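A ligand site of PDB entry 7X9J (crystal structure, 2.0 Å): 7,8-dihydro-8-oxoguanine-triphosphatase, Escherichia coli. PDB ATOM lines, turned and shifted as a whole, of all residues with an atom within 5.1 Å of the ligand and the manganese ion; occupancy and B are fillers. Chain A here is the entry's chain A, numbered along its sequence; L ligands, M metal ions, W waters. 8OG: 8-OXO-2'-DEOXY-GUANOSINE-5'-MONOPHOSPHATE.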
ATOM      1  N   ILE A   6       6.663  25.025  16.690  1.00  0.00           N
ATOM      2  CA  ILE A   6       5.739  25.218  15.570  1.00  0.00           C
ATOM      3  C   ILE A   6       4.541  24.297  15.762  1.00  0.00           C
ATOM      4  O   ILE A   6       4.698  23.099  15.997  1.00  0.00           O
ATOM      5  CB  ILE A   6       6.434  24.913  14.221  1.00  0.00           C
ATOM      6  CG1 ILE A   6       7.736  25.718  14.053  1.00  0.00           C
ATOM      7  CG2 ILE A   6       5.463  25.108  13.067  1.00  0.00           C
ATOM      8  CD1 ILE A   6       7.558  27.240  14.109  1.00  0.00           C
ATOM      9  N   VAL A   8       1.077  22.853  13.852  1.00  0.00           N
ATOM     10  CA  VAL A   8       0.499  22.700  12.518  1.00  0.00           C
ATOM     11  C   VAL A   8      -0.707  21.793  12.639  1.00  0.00           C
ATOM     12  O   VAL A   8      -0.812  20.958  13.549  1.00  0.00           O
ATOM     13  CB  VAL A   8       1.515  22.145  11.478  1.00  0.00           C
ATOM     14  CG1 VAL A   8       2.835  22.926  11.534  1.00  0.00           C
ATOM     15  CG2 VAL A   8       1.774  20.658  11.710  1.00  0.00           C
ATOM     16  N   ARG A  23       4.158  26.555   0.511  1.00  0.00           N
ATOM     17  CA  ARG A  23       4.900  27.665   1.081  1.00  0.00           C
ATOM     18  C   ARG A  23       5.443  28.576  -0.024  1.00  0.00           C
ATOM     19  O   ARG A  23       5.705  28.148  -1.146  1.00  0.00           O
ATOM     20  CB  ARG A  23       6.047  27.127   1.957  1.00  0.00           C
ATOM     21  CG  ARG A  23       5.526  26.263   3.096  1.00  0.00           C
ATOM     22  CD  ARG A  23       6.607  25.707   4.010  1.00  0.00           C
ATOM     23  NE  ARG A  23       7.471  26.756   4.519  1.00  0.00           N
ATOM     24  CZ  ARG A  23       7.233  27.469   5.617  1.00  0.00           C
ATOM     25  NH1 ARG A  23       6.115  27.261   6.312  1.00  0.00           N
ATOM     26  NH2 ARG A  23       8.085  28.404   6.002  1.00  0.00           N
ATOM     27  N   HIS A  28      11.534  30.062   4.306  1.00  0.00           N
ATOM     28  CA  HIS A  28      12.219  28.834   4.698  1.00  0.00           C
ATOM     29  C   HIS A  28      11.388  27.662   4.190  1.00  0.00           C
ATOM     30  O   HIS A  28      10.154  27.722   4.187  1.00  0.00           O
ATOM     31  CB  HIS A  28      12.369  28.778   6.224  1.00  0.00           C
ATOM     32  CG  HIS A  28      13.087  27.558   6.704  1.00  0.00           C
ATOM     33  ND1 HIS A  28      12.466  26.536   7.390  1.00  0.00           N
ATOM     34  CD2 HIS A  28      14.397  27.185   6.598  1.00  0.00           C
ATOM     35  CE1 HIS A  28      13.344  25.585   7.675  1.00  0.00           C
ATOM     36  NE2 HIS A  28      14.524  25.962   7.193  1.00  0.00           N
ATOM     37  N   MET A  29      12.061  26.612   3.734  1.00  0.00           N
ATOM     38  CA  MET A  29      11.393  25.480   3.089  1.00  0.00           C
ATOM     39  C   MET A  29      10.522  25.975   1.934  1.00  0.00           C
ATOM     40  O   MET A  29       9.354  25.611   1.788  1.00  0.00           O
ATOM     41  CB  MET A  29      10.584  24.660   4.105  1.00  0.00           C
ATOM     42  CG  MET A  29      11.462  23.805   5.002  1.00  0.00           C
ATOM     43  SD  MET A  29      12.331  22.530   4.058  1.00  0.00           S
ATOM     44  CE  MET A  29      14.025  23.154   4.079  1.00  0.00           C
ATOM     45  N   GLU A  34       2.799  21.781   2.787  1.00  0.00           N
ATOM     46  CA  GLU A  34       2.841  21.910   4.238  1.00  0.00           C
ATOM     47  C   GLU A  34       1.462  21.686   4.828  1.00  0.00           C
ATOM     48  O   GLU A  34       0.428  21.869   4.178  1.00  0.00           O
ATOM     49  CB  GLU A  34       3.366  23.299   4.660  1.00  0.00           C
ATOM     50  CG  GLU A  34       2.531  24.456   4.096  1.00  0.00           C
ATOM     51  CD  GLU A  34       2.729  25.758   4.860  1.00  0.00           C
ATOM     52  OE1 GLU A  34       3.624  25.860   5.734  1.00  0.00           O
ATOM     53  OE2 GLU A  34       1.971  26.709   4.575  1.00  0.00           O
ATOM     54  N   PHE A  35       1.461  21.291   6.097  1.00  0.00           N
ATOM     55  CA  PHE A  35       0.284  21.468   6.922  1.00  0.00           C
ATOM     56  C   PHE A  35       0.228  22.927   7.403  1.00  0.00           C
ATOM     57  O   PHE A  35       1.246  23.458   7.830  1.00  0.00           O
ATOM     58  CB  PHE A  35       0.336  20.521   8.128  1.00  0.00           C
ATOM     59  CG  PHE A  35       0.560  19.087   7.765  1.00  0.00           C
ATOM     60  CD1 PHE A  35      -0.357  18.402   6.970  1.00  0.00           C
ATOM     61  CD2 PHE A  35       1.681  18.408   8.223  1.00  0.00           C
ATOM     62  CE1 PHE A  35      -0.154  17.073   6.641  1.00  0.00           C
ATOM     63  CE2 PHE A  35       1.879  17.071   7.895  1.00  0.00           C
ATOM     64  CZ  PHE A  35       0.972  16.403   7.099  1.00  0.00           C
ATOM     65  N   PRO A  36      -0.921  23.591   7.318  1.00  0.00           N
ATOM     66  CA  PRO A  36      -0.989  24.976   7.810  1.00  0.00           C
ATOM     67  C   PRO A  36      -0.591  25.042   9.279  1.00  0.00           C
ATOM     68  O   PRO A  36      -0.904  24.147  10.060  1.00  0.00           O
ATOM     69  CB  PRO A  36      -2.452  25.366   7.609  1.00  0.00           C
ATOM     70  CG  PRO A  36      -2.919  24.468   6.490  1.00  0.00           C
ATOM     71  CD  PRO A  36      -2.194  23.164   6.721  1.00  0.00           C
ATOM     72  N   GLY A  37       0.137  26.094   9.650  1.00  0.00           N
ATOM     73  CA  GLY A  37       0.556  26.247  11.026  1.00  0.00           C
ATOM     74  C   GLY A  37       1.590  27.344  11.146  1.00  0.00           C
ATOM     75  O   GLY A  37       1.854  28.063  10.200  1.00  0.00           O
ATOM     76  N   GLY A  38       2.175  27.463  12.333  1.00  0.00           N
ATOM     77  CA  GLY A  38       3.173  28.492  12.545  1.00  0.00           C
ATOM     78  C   GLY A  38       3.666  28.490  13.975  1.00  0.00           C
ATOM     79  O   GLY A  38       3.372  27.585  14.756  1.00  0.00           O
ATOM     80  N   LYS A  39       4.412  29.542  14.314  1.00  0.00           N
ATOM     81  CA  LYS A  39       5.147  29.567  15.577  1.00  0.00           C
ATOM     82  C   LYS A  39       4.208  29.717  16.768  1.00  0.00           C
ATOM     83  O   LYS A  39       3.259  30.511  16.730  1.00  0.00           O
ATOM     84  CB  LYS A  39       6.159  30.705  15.558  1.00  0.00           C
ATOM     85  CG  LYS A  39       7.026  30.782  16.814  1.00  0.00           C
ATOM     86  CD  LYS A  39       7.796  32.096  16.874  1.00  0.00           C
ATOM     87  CE  LYS A  39       8.597  32.200  18.168  1.00  0.00           C
ATOM     88  NZ  LYS A  39       9.250  33.529  18.345  1.00  0.00           N
ATOM     89  N   GLU A  53      -3.354  29.696  14.398  1.00  0.00           N
ATOM     90  CA  GLU A  53      -2.699  29.578  13.102  1.00  0.00           C
ATOM     91  C   GLU A  53      -3.682  29.137  12.009  1.00  0.00           C
ATOM     92  O   GLU A  53      -3.653  29.661  10.893  1.00  0.00           O
ATOM     93  CB  GLU A  53      -1.528  28.602  13.205  1.00  0.00           C
ATOM     94  CG  GLU A  53      -0.310  29.148  13.959  1.00  0.00           C
ATOM     95  CD  GLU A  53       0.404  30.264  13.206  1.00  0.00           C
ATOM     96  OE1 GLU A  53       0.164  30.396  11.991  1.00  0.00           O
ATOM     97  OE2 GLU A  53       1.215  30.990  13.812  1.00  0.00           O
ATOM     98  N   GLU A  57      -4.421  31.265   8.733  1.00  0.00           N
ATOM     99  CA  GLU A  57      -3.911  30.803   7.449  1.00  0.00           C
ATOM    100  C   GLU A  57      -5.020  30.303   6.528  1.00  0.00           C
ATOM    101  O   GLU A  57      -4.966  30.544   5.322  1.00  0.00           O
ATOM    102  CB  GLU A  57      -2.861  29.717   7.653  1.00  0.00           C
ATOM    103  CG  GLU A  57      -1.638  30.201   8.390  1.00  0.00           C
ATOM    104  CD  GLU A  57      -0.361  29.578   7.900  1.00  0.00           C
ATOM    105  OE1 GLU A  57      -0.368  28.400   7.470  1.00  0.00           O
ATOM    106  OE2 GLU A  57       0.671  30.280   7.929  1.00  0.00           O
ATOM    107  N   PHE A  75      17.226  21.540  11.075  1.00  0.00           N
ATOM    108  CA  PHE A  75      17.476  22.066   9.739  1.00  0.00           C
ATOM    109  C   PHE A  75      18.894  22.637   9.687  1.00  0.00           C
ATOM    110  O   PHE A  75      19.548  22.814  10.717  1.00  0.00           O
ATOM    111  CB  PHE A  75      16.441  23.139   9.399  1.00  0.00           C
ATOM    112  CG  PHE A  75      15.091  22.593   9.050  1.00  0.00           C
ATOM    113  CD1 PHE A  75      14.837  22.074   7.780  1.00  0.00           C
ATOM    114  CD2 PHE A  75      14.045  22.653   9.965  1.00  0.00           C
ATOM    115  CE1 PHE A  75      13.572  21.595   7.439  1.00  0.00           C
ATOM    116  CE2 PHE A  75      12.778  22.188   9.628  1.00  0.00           C
ATOM    117  CZ  PHE A  75      12.542  21.647   8.368  1.00  0.00           C
ATOM    118  N   ARG A  78      18.437  26.070  11.639  1.00  0.00           N
ATOM    119  CA  ARG A  78      17.502  26.259  12.736  1.00  0.00           C
ATOM    120  C   ARG A  78      17.035  24.911  13.259  1.00  0.00           C
ATOM    121  O   ARG A  78      17.021  23.909  12.544  1.00  0.00           O
ATOM    122  CB  ARG A  78      16.310  27.118  12.308  1.00  0.00           C
ATOM    123  CG  ARG A  78      15.420  26.486  11.251  1.00  0.00           C
ATOM    124  CD  ARG A  78      14.546  27.535  10.601  1.00  0.00           C
ATOM    125  NE  ARG A  78      15.315  28.394   9.694  1.00  0.00           N
ATOM    126  CZ  ARG A  78      14.880  29.544   9.207  1.00  0.00           C
ATOM    127  NH1 ARG A  78      13.683  30.000   9.540  1.00  0.00           N
ATOM    128  NH2 ARG A  78      15.642  30.261   8.383  1.00  0.00           N
ATOM    129  N   ILE A  80      13.759  23.136  15.049  1.00  0.00           N
ATOM    130  CA  ILE A  80      12.348  23.332  15.311  1.00  0.00           C
ATOM    131  C   ILE A  80      11.743  22.104  15.985  1.00  0.00           C
ATOM    132  O   ILE A  80      12.122  20.964  15.695  1.00  0.00           O
ATOM    133  CB  ILE A  80      11.539  23.682  14.035  1.00  0.00           C
ATOM    134  CG1 ILE A  80      11.332  22.450  13.167  1.00  0.00           C
ATOM    135  CG2 ILE A  80      12.200  24.815  13.243  1.00  0.00           C
ATOM    136  CD1 ILE A  80      10.393  22.708  12.046  1.00  0.00           C
ATOM    137  N   LEU A  82       8.077  20.428  16.205  1.00  0.00           N
ATOM    138  CA  LEU A  82       6.828  20.475  15.446  1.00  0.00           C
ATOM    139  C   LEU A  82       5.745  19.721  16.213  1.00  0.00           C
ATOM    140  O   LEU A  82       5.958  18.568  16.624  1.00  0.00           O
ATOM    141  CB  LEU A  82       7.004  19.878  14.053  1.00  0.00           C
ATOM    142  CG  LEU A  82       7.587  20.766  12.947  1.00  0.00           C
ATOM    143  CD1 LEU A  82       8.250  19.893  11.901  1.00  0.00           C
ATOM    144  CD2 LEU A  82       6.514  21.593  12.296  1.00  0.00           C
ATOM    145  N   PHE A  84       2.210  18.256  15.568  1.00  0.00           N
ATOM    146  CA  PHE A  84       1.292  17.882  14.494  1.00  0.00           C
ATOM    147  C   PHE A  84      -0.039  17.505  15.116  1.00  0.00           C
ATOM    148  O   PHE A  84      -0.167  16.440  15.723  1.00  0.00           O
ATOM    149  CB  PHE A  84       1.833  16.720  13.678  1.00  0.00           C
ATOM    150  CG  PHE A  84       3.097  17.015  12.922  1.00  0.00           C
ATOM    151  CD1 PHE A  84       3.044  17.427  11.591  1.00  0.00           C
ATOM    152  CD2 PHE A  84       4.334  16.839  13.509  1.00  0.00           C
ATOM    153  CE1 PHE A  84       4.219  17.681  10.879  1.00  0.00           C
ATOM    154  CE2 PHE A  84       5.509  17.083  12.806  1.00  0.00           C
ATOM    155  CZ  PHE A  84       5.446  17.513  11.485  1.00  0.00           C
ATOM    156  N   PRO A 116       8.564  19.440   3.816  1.00  0.00           N
ATOM    157  CA  PRO A 116       9.837  19.537   4.517  1.00  0.00           C
ATOM    158  C   PRO A 116      10.249  18.184   5.058  1.00  0.00           C
ATOM    159  O   PRO A 116       9.392  17.352   5.414  1.00  0.00           O
ATOM    160  CB  PRO A 116       9.538  20.529   5.653  1.00  0.00           C
ATOM    161  CG  PRO A 116       8.449  21.403   5.078  1.00  0.00           C
ATOM    162  CD  PRO A 116       7.584  20.402   4.331  1.00  0.00           C
ATOM    163  N   ALA A 118      11.303  17.247   7.780  1.00  0.00           N
ATOM    164  CA  ALA A 118      10.826  16.978   9.139  1.00  0.00           C
ATOM    165  C   ALA A 118       9.492  16.243   9.146  1.00  0.00           C
ATOM    166  O   ALA A 118       9.191  15.581  10.146  1.00  0.00           O
ATOM    167  CB  ALA A 118      10.700  18.293   9.903  1.00  0.00           C
ATOM    168  N   ASN A 119       8.692  16.344   8.080  1.00  0.00           N
ATOM    169  CA  ASN A 119       7.374  15.712   8.035  1.00  0.00           C
ATOM    170  C   ASN A 119       7.401  14.229   7.677  1.00  0.00           C
ATOM    171  O   ASN A 119       6.369  13.566   7.781  1.00  0.00           O
ATOM    172  CB  ASN A 119       6.472  16.450   7.043  1.00  0.00           C
ATOM    173  CG  ASN A 119       6.143  17.867   7.487  1.00  0.00           C
ATOM    174  OD1 ASN A 119       6.896  18.494   8.223  1.00  0.00           O
ATOM    175  ND2 ASN A 119       4.997  18.366   7.056  1.00  0.00           N
HETATM  176  OP3 8OG L   1       7.066  29.807   8.217  1.00  0.00           O
HETATM  177  P   8OG L   1       6.273  29.517   9.451  1.00  0.00           P
HETATM  178  OP1 8OG L   1       5.915  30.681  10.326  1.00  0.00           O
HETATM  179  OP2 8OG L   1       5.123  28.581   9.118  1.00  0.00           O
HETATM  180  O5' 8OG L   1       7.251  28.628  10.371  1.00  0.00           O
HETATM  181  C5' 8OG L   1       7.138  27.213  10.254  1.00  0.00           C
HETATM  182  C4' 8OG L   1       8.504  26.526  10.286  1.00  0.00           C
HETATM  183  O4' 8OG L   1       8.255  25.144  10.492  1.00  0.00           O
HETATM  184  C3' 8OG L   1       9.271  26.631   8.976  1.00  0.00           C
HETATM  185  O3' 8OG L   1      10.675  26.556   9.268  1.00  0.00           O
HETATM  186  C2' 8OG L   1       8.901  25.359   8.245  1.00  0.00           C
HETATM  187  C1' 8OG L   1       8.733  24.363   9.399  1.00  0.00           C
HETATM  188  N9  8OG L   1       7.766  23.320   8.997  1.00  0.00           N
HETATM  189  C8  8OG L   1       8.022  22.033   8.755  1.00  0.00           C
HETATM  190  N7  8OG L   1       6.951  21.306   8.411  1.00  0.00           N
HETATM  191  C5  8OG L   1       5.937  22.209   8.418  1.00  0.00           C
HETATM  192  C6  8OG L   1       4.578  22.110   8.155  1.00  0.00           C
HETATM  193  O6  8OG L   1       4.088  21.003   7.815  1.00  0.00           O
HETATM  194  N1  8OG L   1       3.800  23.204   8.252  1.00  0.00           N
HETATM  195  C2  8OG L   1       4.311  24.391   8.612  1.00  0.00           C
HETATM  196  N2  8OG L   1       3.521  25.481   8.736  1.00  0.00           N
HETATM  197  N3  8OG L   1       5.621  24.530   8.886  1.00  0.00           N
HETATM  198  C4  8OG L   1       6.442  23.457   8.795  1.00  0.00           C
HETATM  199  O8  8OG L   1       9.200  21.537   8.854  1.00  0.00           O
HETATM  200 MN    MN M   1       2.884  29.309   8.598  1.00  0.00          MN
HETATM  201  O   HOH W   1       3.415  31.114   9.671  1.00  0.00           O
HETATM  202  O   HOH W   2       6.614  33.235   9.292  1.00  0.00           O
HETATM  203  O   HOH W   3       6.014  31.155   6.271  1.00  0.00           O
HETATM  204  O   HOH W   4       3.348  30.532   6.470  1.00  0.00           O
HETATM  205  O   HOH W   5       9.755  30.660   8.855  1.00  0.00           O
HETATM  206  O   HOH W   6       2.037  27.695   6.962  1.00  0.00           O
HETATM  207  O   HOH W   7      11.345  28.934  10.521  1.00  0.00           O
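ND1 of His 28 is in hydrogen-bond range of O3' of the ligand, 2.6 Å away.
OD1 of Asn 119 is in hydrogen-bond range of N7 of the ligand (2.8 Å).
N1 of the ligand sits at hydrogen-bond distance from O of Phe 35, at 2.6 Å.
The backbone NH of Phe 35 sits at hydrogen-bond distance from an oxygen (O6) of the ligand.
The guanidinium group (NH2) of Arg 23 lies within salt-bridge range of an oxygen (OP3) of the ligand (2.8 Å).
The side-chain carboxylate (OE1) of Glu 34 is in hydrogen-bond range of a nitrogen (N2) of the ligand.
O of His 28 lies within hydrogen-bond range of NH2 of Arg 23.
NH1 of Arg 23 is in salt-bridge range of OE1 of Glu 34, at 2.9 Å.
Ile 6 touches the ligand (CG1 to O4', 3.6 Å).
CG1 of Val 8 touches N1 of the ligand, 3.4 Å away.
Gly 38 touches the ligand (CA to OP2, 3.9 Å).
Phe 75 touches the ligand (CZ to O8, 3.4 Å).
Ile 80 touches the ligand.
CD1 of Leu 82 touches O8 of the ligand (3.6 Å).
Pro 116 touches the ligand (CB to O8, 3.4 Å).
CB of Ala 118 touches O8 of the ligand, 3.7 Å away.
Within 4 Å of the ligand: Ile 6, Val 8, Arg 23, His 28, Glu 34, Phe 35, Gly 37, Gly 38, Phe 75, Ile 80, Leu 82, Pro 116, Ala 118 and Asn 119.
Of the 21 residues printed, 2 come within 4 Å of the manganese ion.
The manganese ion is bound by water W1 (2.2 Å).
O of Gly 37 is bound to the manganese ion.
An oxygen (OP2) of the ligand binds the manganese ion, at 2.4 Å.
Water W6 binds the manganese ion (2.4 Å).
Water W4 binds the manganese ion (2.5 Å).
The manganese ion is bound by the side-chain carboxylate (OE2) of Glu 57, at 2.5 Å.
The manganese ion has six donor atoms within binding distance.
Water W6 lies within hydrogen-bond range of OE1 of Glu 57, OE2 of Glu 34 and N2 of the ligand.
Water W3 lies within hydrogen-bond range of OP3 of the ligand (2.6 Å) and NH2 of Arg 23 (3.5 Å).
Water W7 lies within hydrogen-bond range of the guanidinium group of Arg 78 (2.8 Å) and an oxygen (O3') of the ligand (2.8 Å).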
